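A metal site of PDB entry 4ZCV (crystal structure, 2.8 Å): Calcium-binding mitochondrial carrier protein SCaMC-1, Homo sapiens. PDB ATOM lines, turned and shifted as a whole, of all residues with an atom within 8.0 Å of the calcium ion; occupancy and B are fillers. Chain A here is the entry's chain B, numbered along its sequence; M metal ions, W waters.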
ATOM      1  N   PHE A  19      -2.399 -13.177  -4.329  1.00  0.00           N
ATOM      2  CA  PHE A  19      -2.161 -12.788  -5.719  1.00  0.00           C
ATOM      3  C   PHE A  19      -1.680 -11.338  -5.813  1.00  0.00           C
ATOM      4  O   PHE A  19      -0.719 -11.043  -6.510  1.00  0.00           O
ATOM      5  CB  PHE A  19      -3.433 -12.989  -6.542  1.00  0.00           C
ATOM      6  CG  PHE A  19      -3.245 -12.747  -8.014  1.00  0.00           C
ATOM      7  CD1 PHE A  19      -2.703 -13.733  -8.825  1.00  0.00           C
ATOM      8  CD2 PHE A  19      -3.626 -11.551  -8.589  1.00  0.00           C
ATOM      9  CE1 PHE A  19      -2.534 -13.523 -10.180  1.00  0.00           C
ATOM     10  CE2 PHE A  19      -3.462 -11.326  -9.939  1.00  0.00           C
ATOM     11  CZ  PHE A  19      -2.920 -12.315 -10.736  1.00  0.00           C
ATOM     12  N   LEU A  22       1.742 -11.017  -4.706  1.00  0.00           N
ATOM     13  CA  LEU A  22       2.678 -11.467  -5.728  1.00  0.00           C
ATOM     14  C   LEU A  22       2.741 -10.550  -6.944  1.00  0.00           C
ATOM     15  O   LEU A  22       3.794 -10.369  -7.554  1.00  0.00           O
ATOM     16  CB  LEU A  22       2.305 -12.886  -6.168  1.00  0.00           C
ATOM     17  CG  LEU A  22       2.440 -13.930  -5.071  1.00  0.00           C
ATOM     18  CD1 LEU A  22       2.111 -15.310  -5.589  1.00  0.00           C
ATOM     19  CD2 LEU A  22       3.841 -13.886  -4.479  1.00  0.00           C
ATOM     20  N   ASP A  23       1.600  -9.963  -7.298  1.00  0.00           N
ATOM     21  CA  ASP A  23       1.496  -9.085  -8.457  1.00  0.00           C
ATOM     22  C   ASP A  23       2.081  -7.692  -8.201  1.00  0.00           C
ATOM     23  O   ASP A  23       1.357  -6.775  -7.823  1.00  0.00           O
ATOM     24  CB  ASP A  23       0.031  -8.978  -8.895  1.00  0.00           C
ATOM     25  CG  ASP A  23      -0.132  -8.252 -10.226  1.00  0.00           C
ATOM     26  OD1 ASP A  23       0.846  -8.200 -11.000  1.00  0.00           O
ATOM     27  OD2 ASP A  23      -1.245  -7.755 -10.491  1.00  0.00           O
ATOM     28  N   ARG A  24       3.380  -7.543  -8.396  1.00  0.00           N
ATOM     29  CA  ARG A  24       4.095  -6.304  -8.067  1.00  0.00           C
ATOM     30  C   ARG A  24       3.668  -5.063  -8.841  1.00  0.00           C
ATOM     31  O   ARG A  24       3.415  -4.012  -8.248  1.00  0.00           O
ATOM     32  CB  ARG A  24       5.587  -6.497  -8.310  1.00  0.00           C
ATOM     33  CG  ARG A  24       6.490  -5.370  -7.805  1.00  0.00           C
ATOM     34  CD  ARG A  24       7.882  -5.555  -8.384  1.00  0.00           C
ATOM     35  NE  ARG A  24       7.843  -5.687  -9.843  1.00  0.00           N
ATOM     36  CZ  ARG A  24       8.883  -5.463 -10.654  1.00  0.00           C
ATOM     37  NH1 ARG A  24      10.061  -5.129 -10.156  1.00  0.00           N
ATOM     38  NH2 ARG A  24       8.751  -5.604 -11.964  1.00  0.00           N
ATOM     39  N   ASN A  25       3.582  -5.186 -10.162  1.00  0.00           N
ATOM     40  CA  ASN A  25       3.259  -4.036 -11.005  1.00  0.00           C
ATOM     41  C   ASN A  25       1.763  -3.829 -11.158  1.00  0.00           C
ATOM     42  O   ASN A  25       1.320  -2.859 -11.780  1.00  0.00           O
ATOM     43  CB  ASN A  25       3.926  -4.206 -12.368  1.00  0.00           C
ATOM     44  CG  ASN A  25       3.473  -5.451 -13.086  1.00  0.00           C
ATOM     45  OD1 ASN A  25       2.981  -6.386 -12.464  1.00  0.00           O
ATOM     46  ND2 ASN A  25       3.651  -5.473 -14.403  1.00  0.00           N
ATOM     47  N   GLY A  26       0.980  -4.746 -10.597  1.00  0.00           N
ATOM     48  CA  GLY A  26      -0.473  -4.622 -10.629  1.00  0.00           C
ATOM     49  C   GLY A  26      -1.033  -4.634 -12.043  1.00  0.00           C
ATOM     50  O   GLY A  26      -1.946  -3.863 -12.352  1.00  0.00           O
ATOM     51  N   ASP A  27      -0.481  -5.483 -12.892  1.00  0.00           N
ATOM     52  CA  ASP A  27      -0.939  -5.578 -14.268  1.00  0.00           C
ATOM     53  C   ASP A  27      -1.988  -6.674 -14.424  1.00  0.00           C
ATOM     54  O   ASP A  27      -2.420  -6.990 -15.522  1.00  0.00           O
ATOM     55  CB  ASP A  27       0.228  -5.824 -15.224  1.00  0.00           C
ATOM     56  CG  ASP A  27       0.951  -7.133 -14.947  1.00  0.00           C
ATOM     57  OD1 ASP A  27       0.703  -7.746 -13.888  1.00  0.00           O
ATOM     58  OD2 ASP A  27       1.762  -7.556 -15.801  1.00  0.00           O
ATOM     59  N   GLY A  28      -2.372  -7.276 -13.299  1.00  0.00           N
ATOM     60  CA  GLY A  28      -3.412  -8.285 -13.287  1.00  0.00           C
ATOM     61  C   GLY A  28      -2.933  -9.710 -13.508  1.00  0.00           C
ATOM     62  O   GLY A  28      -3.726 -10.649 -13.473  1.00  0.00           O
ATOM     63  N   VAL A  29      -1.643  -9.879 -13.767  1.00  0.00           N
ATOM     64  CA  VAL A  29      -1.053 -11.205 -13.915  1.00  0.00           C
ATOM     65  C   VAL A  29       0.229 -11.326 -13.105  1.00  0.00           C
ATOM     66  O   VAL A  29       0.860 -10.323 -12.774  1.00  0.00           O
ATOM     67  CB  VAL A  29      -0.749 -11.547 -15.390  1.00  0.00           C
ATOM     68  CG1 VAL A  29      -2.020 -11.562 -16.221  1.00  0.00           C
ATOM     69  CG2 VAL A  29       0.267 -10.581 -15.956  1.00  0.00           C
ATOM     70  N   VAL A  30       0.621 -12.559 -12.795  1.00  0.00           N
ATOM     71  CA  VAL A  30       1.858 -12.825 -12.089  1.00  0.00           C
ATOM     72  C   VAL A  30       2.859 -13.534 -12.994  1.00  0.00           C
ATOM     73  O   VAL A  30       2.600 -14.638 -13.472  1.00  0.00           O
ATOM     74  CB  VAL A  30       1.621 -13.668 -10.821  1.00  0.00           C
ATOM     75  CG1 VAL A  30       2.937 -14.169 -10.252  1.00  0.00           C
ATOM     76  CG2 VAL A  30       0.855 -12.872  -9.783  1.00  0.00           C
ATOM     77  N   ASP A  31       4.001 -12.898 -13.239  1.00  0.00           N
ATOM     78  CA  ASP A  31       5.062 -13.522 -14.015  1.00  0.00           C
ATOM     79  C   ASP A  31       6.017 -14.283 -13.095  1.00  0.00           C
ATOM     80  O   ASP A  31       5.979 -14.135 -11.875  1.00  0.00           O
ATOM     81  CB  ASP A  31       5.816 -12.475 -14.846  1.00  0.00           C
ATOM     82  CG  ASP A  31       6.248 -11.280 -14.033  1.00  0.00           C
ATOM     83  OD1 ASP A  31       7.222 -11.402 -13.267  1.00  0.00           O
ATOM     84  OD2 ASP A  31       5.615 -10.209 -14.158  1.00  0.00           O
ATOM     85  N   ILE A  32       6.886 -15.108 -13.693  1.00  0.00           N
ATOM     86  CA  ILE A  32       7.762 -15.989 -12.906  1.00  0.00           C
ATOM     87  C   ILE A  32       8.702 -15.200 -11.990  1.00  0.00           C
ATOM     88  O   ILE A  32       8.985 -15.619 -10.862  1.00  0.00           O
ATOM     89  CB  ILE A  32       8.584 -16.930 -13.835  1.00  0.00           C
ATOM     90  CG1 ILE A  32       9.339 -17.974 -13.015  1.00  0.00           C
ATOM     91  CG2 ILE A  32       9.498 -16.142 -14.768  1.00  0.00           C
ATOM     92  CD1 ILE A  32       8.423 -18.873 -12.192  1.00  0.00           C
ATOM     93  N   GLU A  34       8.014 -12.259 -10.673  1.00  0.00           N
ATOM     94  CA  GLU A  34       7.156 -11.798  -9.591  1.00  0.00           C
ATOM     95  C   GLU A  34       6.862 -12.914  -8.587  1.00  0.00           C
ATOM     96  O   GLU A  34       6.729 -12.654  -7.395  1.00  0.00           O
ATOM     97  CB  GLU A  34       5.848 -11.252 -10.154  1.00  0.00           C
ATOM     98  CG  GLU A  34       5.971  -9.865 -10.748  1.00  0.00           C
ATOM     99  CD  GLU A  34       4.672  -9.384 -11.339  1.00  0.00           C
ATOM    100  OE1 GLU A  34       3.801 -10.240 -11.595  1.00  0.00           O
ATOM    101  OE2 GLU A  34       4.504  -8.159 -11.525  1.00  0.00           O
ATOM    102  N   LEU A  35       6.760 -14.143  -9.078  1.00  0.00           N
ATOM    103  CA  LEU A  35       6.513 -15.284  -8.209  1.00  0.00           C
ATOM    104  C   LEU A  35       7.716 -15.574  -7.325  1.00  0.00           C
ATOM    105  O   LEU A  35       7.564 -15.804  -6.125  1.00  0.00           O
ATOM    106  CB  LEU A  35       6.165 -16.533  -9.027  1.00  0.00           C
ATOM    107  CG  LEU A  35       5.826 -17.764  -8.184  1.00  0.00           C
ATOM    108  CD1 LEU A  35       4.572 -17.551  -7.363  1.00  0.00           C
ATOM    109  CD2 LEU A  35       5.702 -19.005  -9.065  1.00  0.00           C
ATOM    110  N   LYS A  65       2.086 -16.692 -18.415  1.00  0.00           N
ATOM    111  CA  LYS A  65       1.637 -15.806 -17.349  1.00  0.00           C
ATOM    112  C   LYS A  65       0.552 -16.468 -16.499  1.00  0.00           C
ATOM    113  O   LYS A  65      -0.183 -17.332 -16.968  1.00  0.00           O
ATOM    114  CB  LYS A  65       1.118 -14.473 -17.914  1.00  0.00           C
ATOM    115  CG  LYS A  65       2.111 -13.746 -18.816  1.00  0.00           C
ATOM    116  CD  LYS A  65       1.520 -12.457 -19.392  1.00  0.00           C
ATOM    117  CE  LYS A  65       0.451 -12.706 -20.437  1.00  0.00           C
ATOM    118  NZ  LYS A  65       1.027 -13.255 -21.695  1.00  0.00           N
ATOM    119  N   LEU A  66       0.462 -16.051 -15.243  1.00  0.00           N
ATOM    120  CA  LEU A  66      -0.592 -16.525 -14.356  1.00  0.00           C
ATOM    121  C   LEU A  66      -1.589 -15.411 -14.071  1.00  0.00           C
ATOM    122  O   LEU A  66      -1.286 -14.492 -13.312  1.00  0.00           O
ATOM    123  CB  LEU A  66      -0.004 -17.026 -13.032  1.00  0.00           C
ATOM    124  CG  LEU A  66       0.713 -18.375 -13.005  1.00  0.00           C
ATOM    125  CD1 LEU A  66       1.220 -18.674 -11.599  1.00  0.00           C
ATOM    126  CD2 LEU A  66      -0.205 -19.482 -13.487  1.00  0.00           C
HETATM  127 CA    CA M   1       2.450  -8.624 -12.700  1.00  0.00          CA
HETATM  128  O   HOH W   1       3.709  -8.918 -14.646  1.00  0.00           O
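Water W1 lies within hydrogen-bond range of OD2 of Asp 27 (2.6 Å) and ND2 of Asn 25 (3.5 Å).
The side-chain carboxylate (OD1) of Asp 27 binds the calcium ion, at 2.3 Å. The calcium ion is bound by OD1 of Asn 25, at 2.3 Å. The backbone carbonyl oxygen (O) of Val 29 is bound to the calcium ion (2.3 Å). The calcium ion is bound by water W1 (2.3 Å). The calcium ion is bound by the side-chain carboxylate (OD1) of Asp 23 (2.4 Å). OE1 of Glu 34 is bound to the calcium ion (2.4 Å). OE2 of Glu 34 binds the calcium ion (2.4 Å). The calcium ion has seven donor atoms within binding distance.
The backbone NH (N) of Arg 24 lies close to the side-chain carboxylate (OE2) of Glu 34 (3.4 Å). The side-chain carboxylate of Asp 23 lies close to the backbone NH of Gly 26. The side-chain carboxylate (OD2) of Asp 23 lies within hydrogen-bond range of the backbone NH (N) of Gly 28 (3.1 Å). N of Glu 34 lies within hydrogen-bond range of OD1 of Asp 31, 2.8 Å away.
Merely in contact with the calcium ion: Asp 31 (3.8 Å). Six residues have an atom within 4 Å of the calcium ion: Asp 23, Asn 25, Asp 27, Val 29, Asp 31 and Glu 34. Along chain A the residues within 4 Å of the calcium ion span positions 23 to 34. The nearest printed residue that does not touch the calcium ion is Val 30 (4.3 Å).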
